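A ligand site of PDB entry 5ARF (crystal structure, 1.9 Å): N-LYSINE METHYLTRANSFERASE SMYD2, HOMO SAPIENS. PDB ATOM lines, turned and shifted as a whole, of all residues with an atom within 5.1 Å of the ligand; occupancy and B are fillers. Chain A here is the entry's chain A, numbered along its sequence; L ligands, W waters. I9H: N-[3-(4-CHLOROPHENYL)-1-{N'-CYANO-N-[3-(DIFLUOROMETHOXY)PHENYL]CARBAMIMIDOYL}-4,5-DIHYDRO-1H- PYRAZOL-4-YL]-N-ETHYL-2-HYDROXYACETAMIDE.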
ATOM      1  N   VAL A  42       0.590  18.740   0.491  1.00  0.00           N
ATOM      2  CA  VAL A  42       0.852  19.416   1.737  1.00  0.00           C
ATOM      3  C   VAL A  42       0.012  20.684   1.776  1.00  0.00           C
ATOM      4  O   VAL A  42      -0.112  21.421   0.757  1.00  0.00           O
ATOM      5  CB  VAL A  42       2.363  19.699   1.874  1.00  0.00           C
ATOM      6  CG1 VAL A  42       2.858  20.734   0.870  1.00  0.00           C
ATOM      7  CG2 VAL A  42       2.700  20.179   3.261  1.00  0.00           C
ATOM      8  N   GLU A 104       8.110  24.976   0.864  1.00  0.00           N
ATOM      9  CA  GLU A 104       6.980  24.075   0.605  1.00  0.00           C
ATOM     10  C   GLU A 104       7.467  22.899  -0.253  1.00  0.00           C
ATOM     11  O   GLU A 104       7.074  21.741  -0.069  1.00  0.00           O
ATOM     12  CB  GLU A 104       5.841  24.855   0.003  1.00  0.00           C
ATOM     13  CG  GLU A 104       4.560  24.089  -0.053  1.00  0.00           C
ATOM     14  CD  GLU A 104       3.385  25.000  -0.021  1.00  0.00           C
ATOM     15  OE1 GLU A 104       3.328  25.914   0.864  1.00  0.00           O
ATOM     16  OE2 GLU A 104       2.554  24.853  -0.964  1.00  0.00           O
ATOM     17  N   THR A 105       8.402  23.225  -1.138  1.00  0.00           N
ATOM     18  CA  THR A 105       9.047  22.226  -1.958  1.00  0.00           C
ATOM     19  C   THR A 105       9.736  21.162  -1.167  1.00  0.00           C
ATOM     20  O   THR A 105       9.604  19.986  -1.465  1.00  0.00           O
ATOM     21  CB  THR A 105       9.997  22.868  -2.965  1.00  0.00           C
ATOM     22  OG1 THR A 105       9.213  23.716  -3.826  1.00  0.00           O
ATOM     23  CG2 THR A 105      10.729  21.812  -3.781  1.00  0.00           C
ATOM     24  N   LEU A 108       6.947  18.968   0.553  1.00  0.00           N
ATOM     25  CA  LEU A 108       6.273  18.031  -0.363  1.00  0.00           C
ATOM     26  C   LEU A 108       7.162  16.874  -0.730  1.00  0.00           C
ATOM     27  O   LEU A 108       6.726  15.751  -0.797  1.00  0.00           O
ATOM     28  CB  LEU A 108       5.792  18.780  -1.623  1.00  0.00           C
ATOM     29  CG  LEU A 108       4.934  17.944  -2.599  1.00  0.00           C
ATOM     30  CD1 LEU A 108       3.655  17.435  -1.984  1.00  0.00           C
ATOM     31  CD2 LEU A 108       4.659  18.667  -3.926  1.00  0.00           C
ATOM     32  N   VAL A 179       9.990  17.035  -9.386  1.00  0.00           N
ATOM     33  CA  VAL A 179       9.025  17.873  -8.640  1.00  0.00           C
ATOM     34  C   VAL A 179       8.818  19.252  -9.314  1.00  0.00           C
ATOM     35  O   VAL A 179       7.718  19.693  -9.477  1.00  0.00           O
ATOM     36  CB  VAL A 179       9.411  18.035  -7.141  1.00  0.00           C
ATOM     37  CG1 VAL A 179       8.542  19.044  -6.392  1.00  0.00           C
ATOM     38  CG2 VAL A 179       9.249  16.683  -6.473  1.00  0.00           C
ATOM     39  N   ASN A 180       9.889  19.892  -9.674  1.00  0.00           N
ATOM     40  CA  ASN A 180       9.726  21.181 -10.337  1.00  0.00           C
ATOM     41  C   ASN A 180       9.020  21.067 -11.714  1.00  0.00           C
ATOM     42  O   ASN A 180       8.320  21.980 -12.126  1.00  0.00           O
ATOM     43  CB  ASN A 180      11.117  21.894 -10.438  1.00  0.00           C
ATOM     44  CG  ASN A 180      11.557  22.489  -9.097  1.00  0.00           C
ATOM     45  OD1 ASN A 180      10.723  22.820  -8.181  1.00  0.00           O
ATOM     46  ND2 ASN A 180      12.862  22.626  -8.949  1.00  0.00           N
ATOM     47  N   CYS A 181       9.250  19.945 -12.414  1.00  0.00           N
ATOM     48  CA  CYS A 181       8.714  19.770 -13.786  1.00  0.00           C
ATOM     49  C   CYS A 181       7.246  19.302 -13.722  1.00  0.00           C
ATOM     50  O   CYS A 181       6.516  19.473 -14.663  1.00  0.00           O
ATOM     51  CB  CYS A 181       9.583  18.756 -14.557  1.00  0.00           C
ATOM     52  SG  CYS A 181       9.037  18.439 -16.278  1.00  0.00           S
ATOM     53  N   ASN A 182       6.832  18.718 -12.585  1.00  0.00           N
ATOM     54  CA  ASN A 182       5.577  17.986 -12.557  1.00  0.00           C
ATOM     55  C   ASN A 182       4.638  18.312 -11.375  1.00  0.00           C
ATOM     56  O   ASN A 182       3.489  17.902 -11.387  1.00  0.00           O
ATOM     57  CB  ASN A 182       5.828  16.499 -12.538  1.00  0.00           C
ATOM     58  CG  ASN A 182       6.563  16.018 -13.768  1.00  0.00           C
ATOM     59  OD1 ASN A 182       7.818  15.862 -13.779  1.00  0.00           O
ATOM     60  ND2 ASN A 182       5.797  15.758 -14.814  1.00  0.00           N
ATOM     61  N   GLY A 183       5.166  18.977 -10.360  1.00  0.00           N
ATOM     62  CA  GLY A 183       4.328  19.379  -9.204  1.00  0.00           C
ATOM     63  C   GLY A 183       3.260  20.370  -9.575  1.00  0.00           C
ATOM     64  O   GLY A 183       3.381  21.083 -10.593  1.00  0.00           O
ATOM     65  N   PHE A 184       2.240  20.472  -8.690  1.00  0.00           N
ATOM     66  CA  PHE A 184       1.119  21.380  -8.830  1.00  0.00           C
ATOM     67  C   PHE A 184       0.973  22.227  -7.582  1.00  0.00           C
ATOM     68  O   PHE A 184       1.325  21.756  -6.517  1.00  0.00           O
ATOM     69  CB  PHE A 184      -0.204  20.607  -8.912  1.00  0.00           C
ATOM     70  CG  PHE A 184      -0.416  19.882 -10.193  1.00  0.00           C
ATOM     71  CD1 PHE A 184       0.215  18.677 -10.411  1.00  0.00           C
ATOM     72  CD2 PHE A 184      -1.241  20.439 -11.189  1.00  0.00           C
ATOM     73  CE1 PHE A 184       0.096  18.027 -11.626  1.00  0.00           C
ATOM     74  CE2 PHE A 184      -1.382  19.788 -12.399  1.00  0.00           C
ATOM     75  CZ  PHE A 184      -0.710  18.609 -12.633  1.00  0.00           C
ATOM     76  N   THR A 185       0.392  23.412  -7.717  1.00  0.00           N
ATOM     77  CA  THR A 185      -0.246  24.106  -6.594  1.00  0.00           C
ATOM     78  C   THR A 185      -1.692  23.773  -6.537  1.00  0.00           C
ATOM     79  O   THR A 185      -2.314  23.534  -7.574  1.00  0.00           O
ATOM     80  CB  THR A 185      -0.115  25.624  -6.681  1.00  0.00           C
ATOM     81  OG1 THR A 185      -0.897  26.091  -7.781  1.00  0.00           O
ATOM     82  CG2 THR A 185       1.314  25.950  -6.819  1.00  0.00           C
ATOM     83  N   ILE A 186      -2.234  23.697  -5.328  1.00  0.00           N
ATOM     84  CA  ILE A 186      -3.680  23.686  -5.165  1.00  0.00           C
ATOM     85  C   ILE A 186      -4.124  25.110  -4.688  1.00  0.00           C
ATOM     86  O   ILE A 186      -3.603  25.677  -3.712  1.00  0.00           O
ATOM     87  CB  ILE A 186      -4.133  22.607  -4.210  1.00  0.00           C
ATOM     88  CG1 ILE A 186      -3.732  21.229  -4.765  1.00  0.00           C
ATOM     89  CG2 ILE A 186      -5.624  22.744  -3.782  1.00  0.00           C
ATOM     90  CD1 ILE A 186      -4.030  20.146  -3.810  1.00  0.00           C
ATOM     91  N   GLU A 187      -5.034  25.712  -5.461  1.00  0.00           N
ATOM     92  CA  GLU A 187      -5.652  27.008  -5.163  1.00  0.00           C
ATOM     93  C   GLU A 187      -7.158  26.915  -4.963  1.00  0.00           C
ATOM     94  O   GLU A 187      -7.824  26.044  -5.559  1.00  0.00           O
ATOM     95  CB  GLU A 187      -5.298  27.967  -6.287  1.00  0.00           C
ATOM     96  CG  GLU A 187      -3.780  28.064  -6.493  1.00  0.00           C
ATOM     97  CD  GLU A 187      -3.370  28.442  -7.904  1.00  0.00           C
ATOM     98  OE1 GLU A 187      -4.167  28.295  -8.879  1.00  0.00           O
ATOM     99  OE2 GLU A 187      -2.232  28.952  -8.019  1.00  0.00           O
ATOM    100  N   SER A 196       0.300  22.457  -2.160  1.00  0.00           N
ATOM    101  CA  SER A 196       1.107  21.959  -3.299  1.00  0.00           C
ATOM    102  C   SER A 196       0.901  20.461  -3.254  1.00  0.00           C
ATOM    103  O   SER A 196       0.624  19.869  -2.162  1.00  0.00           O
ATOM    104  CB  SER A 196       2.572  22.383  -3.225  1.00  0.00           C
ATOM    105  OG  SER A 196       2.799  23.795  -3.361  1.00  0.00           O
ATOM    106  N   ALA A 197       1.017  19.837  -4.415  1.00  0.00           N
ATOM    107  CA  ALA A 197       0.663  18.423  -4.577  1.00  0.00           C
ATOM    108  C   ALA A 197       1.244  17.744  -5.868  1.00  0.00           C
ATOM    109  O   ALA A 197       1.700  18.404  -6.801  1.00  0.00           O
ATOM    110  CB  ALA A 197      -0.831  18.202  -4.522  1.00  0.00           C
ATOM    111  N   VAL A 202      -2.311  13.524 -14.028  1.00  0.00           N
ATOM    112  CA  VAL A 202      -2.554  14.827 -14.533  1.00  0.00           C
ATOM    113  C   VAL A 202      -1.300  15.421 -15.172  1.00  0.00           C
ATOM    114  O   VAL A 202      -1.414  16.201 -16.137  1.00  0.00           O
ATOM    115  CB  VAL A 202      -3.178  15.764 -13.425  1.00  0.00           C
ATOM    116  CG1 VAL A 202      -3.588  17.125 -13.984  1.00  0.00           C
ATOM    117  CG2 VAL A 202      -4.353  15.102 -12.734  1.00  0.00           C
ATOM    118  N   ALA A 203      -0.111  15.069 -14.671  1.00  0.00           N
ATOM    119  CA  ALA A 203       1.125  15.638 -15.171  1.00  0.00           C
ATOM    120  C   ALA A 203       1.551  15.056 -16.498  1.00  0.00           C
ATOM    121  O   ALA A 203       2.502  15.479 -17.038  1.00  0.00           O
ATOM    122  CB  ALA A 203       2.295  15.504 -14.183  1.00  0.00           C
ATOM    123  N   MET A 205      -0.251  15.421 -19.083  1.00  0.00           N
ATOM    124  CA  MET A 205      -0.799  16.363 -20.034  1.00  0.00           C
ATOM    125  C   MET A 205       0.195  17.437 -20.323  1.00  0.00           C
ATOM    126  O   MET A 205       0.781  18.024 -19.438  1.00  0.00           O
ATOM    127  CB  MET A 205      -2.091  17.037 -19.563  1.00  0.00           C
ATOM    128  CG  MET A 205      -3.315  16.143 -19.503  1.00  0.00           C
ATOM    129  SD  MET A 205      -4.841  16.982 -19.004  1.00  0.00           S
ATOM    130  CE  MET A 205      -4.497  17.608 -17.349  1.00  0.00           C
ATOM    131  N   TYR A 217      -9.781  21.543  -8.352  1.00  0.00           N
ATOM    132  CA  TYR A 217      -9.495  20.656  -7.179  1.00  0.00           C
ATOM    133  C   TYR A 217     -10.748  20.539  -6.350  1.00  0.00           C
ATOM    134  O   TYR A 217     -11.456  21.492  -6.189  1.00  0.00           O
ATOM    135  CB  TYR A 217      -8.290  21.188  -6.374  1.00  0.00           C
ATOM    136  CG  TYR A 217      -7.113  21.447  -7.262  1.00  0.00           C
ATOM    137  CD1 TYR A 217      -6.284  20.389  -7.670  1.00  0.00           C
ATOM    138  CD2 TYR A 217      -6.824  22.714  -7.718  1.00  0.00           C
ATOM    139  CE1 TYR A 217      -5.211  20.589  -8.545  1.00  0.00           C
ATOM    140  CE2 TYR A 217      -5.720  22.927  -8.532  1.00  0.00           C
ATOM    141  CZ  TYR A 217      -4.932  21.864  -8.980  1.00  0.00           C
ATOM    142  OH  TYR A 217      -3.897  22.148  -9.837  1.00  0.00           O
ATOM    143  N   THR A 238      -3.663  21.069 -21.115  1.00  0.00           N
ATOM    144  CA  THR A 238      -4.027  22.039 -20.092  1.00  0.00           C
ATOM    145  C   THR A 238      -3.046  23.184 -20.191  1.00  0.00           C
ATOM    146  O   THR A 238      -2.058  23.092 -20.885  1.00  0.00           O
ATOM    147  CB  THR A 238      -3.958  21.422 -18.669  1.00  0.00           C
ATOM    148  OG1 THR A 238      -4.540  22.345 -17.749  1.00  0.00           O
ATOM    149  CG2 THR A 238      -2.486  21.077 -18.275  1.00  0.00           C
ATOM    150  N   SER A 239      -3.255  24.224 -19.417  1.00  0.00           N
ATOM    151  CA  SER A 239      -2.286  25.301 -19.344  1.00  0.00           C
ATOM    152  C   SER A 239      -1.401  25.225 -18.094  1.00  0.00           C
ATOM    153  O   SER A 239      -1.915  24.982 -16.989  1.00  0.00           O
ATOM    154  CB  SER A 239      -3.012  26.601 -19.298  1.00  0.00           C
ATOM    155  OG  SER A 239      -2.149  27.647 -19.067  1.00  0.00           O
ATOM    156  N   TYR A 240      -0.097  25.487 -18.249  1.00  0.00           N
ATOM    157  CA  TYR A 240       0.827  25.406 -17.117  1.00  0.00           C
ATOM    158  C   TYR A 240       0.967  26.790 -16.458  1.00  0.00           C
ATOM    159  O   TYR A 240       1.609  26.936 -15.377  1.00  0.00           O
ATOM    160  CB  TYR A 240       2.219  24.895 -17.529  1.00  0.00           C
ATOM    161  CG  TYR A 240       2.346  23.457 -18.052  1.00  0.00           C
ATOM    162  CD1 TYR A 240       1.267  22.598 -18.110  1.00  0.00           C
ATOM    163  CD2 TYR A 240       3.571  22.983 -18.464  1.00  0.00           C
ATOM    164  CE1 TYR A 240       1.409  21.314 -18.591  1.00  0.00           C
ATOM    165  CE2 TYR A 240       3.746  21.673 -18.943  1.00  0.00           C
ATOM    166  CZ  TYR A 240       2.648  20.851 -19.000  1.00  0.00           C
ATOM    167  OH  TYR A 240       2.748  19.577 -19.454  1.00  0.00           O
ATOM    168  N   ILE A 241       0.400  27.806 -17.091  1.00  0.00           N
ATOM    169  CA  ILE A 241       0.705  29.155 -16.690  1.00  0.00           C
ATOM    170  C   ILE A 241      -0.466  30.090 -16.740  1.00  0.00           C
ATOM    171  O   ILE A 241      -1.550  29.823 -17.326  1.00  0.00           O
ATOM    172  CB  ILE A 241       1.836  29.734 -17.577  1.00  0.00           C
ATOM    173  CG1 ILE A 241       1.406  29.630 -19.076  1.00  0.00           C
ATOM    174  CG2 ILE A 241       3.179  29.061 -17.288  1.00  0.00           C
ATOM    175  CD1 ILE A 241       2.273  30.373 -20.097  1.00  0.00           C
ATOM    176  N   ASP A 242      -0.236  31.272 -16.182  1.00  0.00           N
ATOM    177  CA  ASP A 242      -1.187  32.381 -16.331  1.00  0.00           C
ATOM    178  C   ASP A 242      -1.219  32.914 -17.773  1.00  0.00           C
ATOM    179  O   ASP A 242      -0.238  33.472 -18.270  1.00  0.00           O
ATOM    180  CB  ASP A 242      -0.788  33.492 -15.349  1.00  0.00           C
ATOM    181  CG  ASP A 242      -1.875  34.582 -15.164  1.00  0.00           C
ATOM    182  OD1 ASP A 242      -2.716  34.806 -16.077  1.00  0.00           O
ATOM    183  OD2 ASP A 242      -1.912  35.205 -14.081  1.00  0.00           O
ATOM    184  N   TYR A 258       9.842  24.929 -17.630  1.00  0.00           N
ATOM    185  CA  TYR A 258       9.536  23.603 -18.229  1.00  0.00           C
ATOM    186  C   TYR A 258      10.417  23.198 -19.403  1.00  0.00           C
ATOM    187  O   TYR A 258      10.193  22.154 -20.020  1.00  0.00           O
ATOM    188  CB  TYR A 258       8.052  23.543 -18.623  1.00  0.00           C
ATOM    189  CG  TYR A 258       7.167  23.744 -17.417  1.00  0.00           C
ATOM    190  CD1 TYR A 258       6.942  22.676 -16.524  1.00  0.00           C
ATOM    191  CD2 TYR A 258       6.615  24.989 -17.102  1.00  0.00           C
ATOM    192  CE1 TYR A 258       6.188  22.844 -15.379  1.00  0.00           C
ATOM    193  CE2 TYR A 258       5.850  25.164 -15.922  1.00  0.00           C
ATOM    194  CZ  TYR A 258       5.614  24.083 -15.081  1.00  0.00           C
ATOM    195  OH  TYR A 258       4.871  24.198 -13.897  1.00  0.00           O
HETATM  196  CAG I9H L   1       1.868  21.707 -13.421  1.00  0.00           C
HETATM  197  CAL I9H L   1       1.590  20.615 -14.247  1.00  0.00           C
HETATM  198  CAR I9H L   1       0.484  20.740 -15.137  1.00  0.00           C
HETATM  199 CL1  I9H L   1       0.159  19.371 -16.083  1.00  0.00          CL
HETATM  200  CAM I9H L   1      -0.301  21.877 -15.132  1.00  0.00           C
HETATM  201  CAH I9H L   1       0.039  22.934 -14.303  1.00  0.00           C
HETATM  202  CAC I9H L   1       1.117  22.849 -13.426  1.00  0.00           C
HETATM  203  CAA I9H L   1       1.508  23.874 -12.580  1.00  0.00           C
HETATM  204  NAD I9H L   1       2.440  23.816 -11.609  1.00  0.00           N
HETATM  205  CAB I9H L   1       1.006  25.289 -12.652  1.00  0.00           C
HETATM  206  NAF I9H L   1      -0.488  25.517 -12.360  1.00  0.00           N
HETATM  207  CAK I9H L   1      -1.214  26.462 -13.307  1.00  0.00           C
HETATM  208  CAQ I9H L   1      -1.007  27.942 -13.004  1.00  0.00           C
HETATM  209  CAJ I9H L   1      -1.037  25.042 -11.221  1.00  0.00           C
HETATM  210  OAP I9H L   1      -0.415  24.246 -10.514  1.00  0.00           O
HETATM  211  CAO I9H L   1      -2.505  25.469 -10.859  1.00  0.00           C
HETATM  212  OAU I9H L   1      -3.168  24.594  -9.886  1.00  0.00           O
HETATM  213  CAE I9H L   1       1.752  25.991 -11.578  1.00  0.00           C
HETATM  214  NAI I9H L   1       2.653  24.933 -11.087  1.00  0.00           N
HETATM  215  CAN I9H L   1       3.440  25.046  -9.980  1.00  0.00           C
HETATM  216  NAT I9H L   1       3.618  26.238  -9.369  1.00  0.00           N
HETATM  217  CAX I9H L   1       4.332  26.397  -8.209  1.00  0.00           C
HETATM  218  NBA I9H L   1       4.936  26.535  -7.217  1.00  0.00           N
HETATM  219  NAS I9H L   1       3.841  23.822  -9.552  1.00  0.00           N
HETATM  220  CAW I9H L   1       4.855  23.566  -8.697  1.00  0.00           C
HETATM  221  CAY I9H L   1       4.623  22.940  -7.496  1.00  0.00           C
HETATM  222  CAZ I9H L   1       6.191  23.885  -9.044  1.00  0.00           C
HETATM  223  CBC I9H L   1       7.270  23.606  -8.170  1.00  0.00           C
HETATM  224  CBD I9H L   1       7.010  22.929  -6.962  1.00  0.00           C
HETATM  225  CBB I9H L   1       5.677  22.617  -6.621  1.00  0.00           C
HETATM  226  OBE I9H L   1       5.355  21.970  -5.439  1.00  0.00           O
HETATM  227  CBF I9H L   1       6.294  22.234  -4.311  1.00  0.00           C
HETATM  228  FBH I9H L   1       5.598  22.025  -3.150  1.00  0.00           F
HETATM  229  FBG I9H L   1       7.153  21.289  -4.492  1.00  0.00           F
HETATM  230  O   HOH W   1      -3.278  29.708 -14.861  1.00  0.00           O
HETATM  231  O   HOH W   2      -3.453  22.926 -15.511  1.00  0.00           O
HETATM  232  O   HOH W   3      -5.778  24.889 -12.079  1.00  0.00           O
HETATM  233  O   HOH W   4      -3.464  27.091 -15.814  1.00  0.00           O
HETATM  234  O   HOH W   5       4.594  25.338  -4.379  1.00  0.00           O
HETATM  235  O   HOH W   6      -3.468  23.177 -12.867  1.00  0.00           O
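Water W5 lies within hydrogen-bond range of OG of Ser 196 (2.6 Å) and NBA of the ligand (3.1 Å).
Water W6 bridges the side-chain hydroxyl of Tyr 217 (3.2 Å) and an oxygen (OAU) of the ligand (3.3 Å).
Water W2 lies within hydrogen-bond range of the side-chain hydroxyl (OG1) of Thr 238 (2.6 Å) and the backbone carbonyl oxygen (O) of Ser 239 (3.0 Å).
An oxygen (OAU) of the ligand is in hydrogen-bond range of the backbone carbonyl oxygen of Thr 185.
The backbone carbonyl oxygen (O) of Gly 183 sits at hydrogen-bond distance from a nitrogen (NAS) of the ligand (3.0 Å).
An oxygen (OAP) of the ligand is in hydrogen-bond range of the backbone NH (N) of Thr 185 (3.0 Å).
The side-chain hydroxyl (OG1) of Thr 185 is in hydrogen-bond range of an oxygen (OAP) of the ligand (3.3 Å).
The side-chain hydroxyl (OH) of Tyr 258 sits at hydrogen-bond distance from a nitrogen (NAD) of the ligand (3.4 Å).
The side-chain hydroxyl (OH) of Tyr 217 sits at hydrogen-bond distance from an oxygen (OAU) of the ligand.
The backbone carbonyl oxygen of Ile 241 lies within hydrogen-bond range of the side-chain hydroxyl of Ser 239, 2.9 Å away.
The side-chain hydroxyl (OG) of Ser 196 is in hydrogen-bond range of the side-chain carboxylate (OE2) of Glu 104 (2.6 Å).
The backbone carbonyl oxygen of Met 205 lies within hydrogen-bond range of the side-chain hydroxyl of Tyr 240 (2.5 Å).
O of Thr 185 is in hydrogen-bond range of OH of Tyr 217.
O of Ser 196 sits at hydrogen-bond distance from N of Val 42.
N of Phe 184 lies within hydrogen-bond range of O of Ala 197 (2.9 Å).
OG1 of Thr 185 is in hydrogen-bond range of OE2 of Glu 187, at 3.2 Å.
The backbone carbonyl oxygen (O) of Glu 104 lies close to a fluorine (FBH) of the ligand (3.4 Å).
The side-chain hydroxyl (OG1) of Thr 105 sits close to a fluorine (FBG) of the ligand, at 3.3 Å.
FBH of the ligand lies close to OG of Ser 196 (3.3 Å).
Merely in contact with the ligand: Tyr 240 (3.2 Å), Val 179 (3.3 Å), Phe 184 (3.4 Å), Val 202 (3.5 Å), Asn 180 (3.5 Å), Leu 108 (3.6 Å), Met 205 (3.7 Å), Glu 187 (3.8 Å), Thr 238 (3.8 Å), Ser 239 (3.9 Å) and Ala 203 (3.96 Å).
18 residues have an atom within 4 Å of the ligand: Glu 104, Thr 105, Leu 108, Val 179, Asn 180, Gly 183, Phe 184, Thr 185, Glu 187, Ser 196, Val 202, Ala 203, Met 205, Tyr 217, Thr 238, Ser 239, Tyr 240 and Tyr 258.
The nearest printed residue that does not touch the ligand is Ile 241 (4.2 Å).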
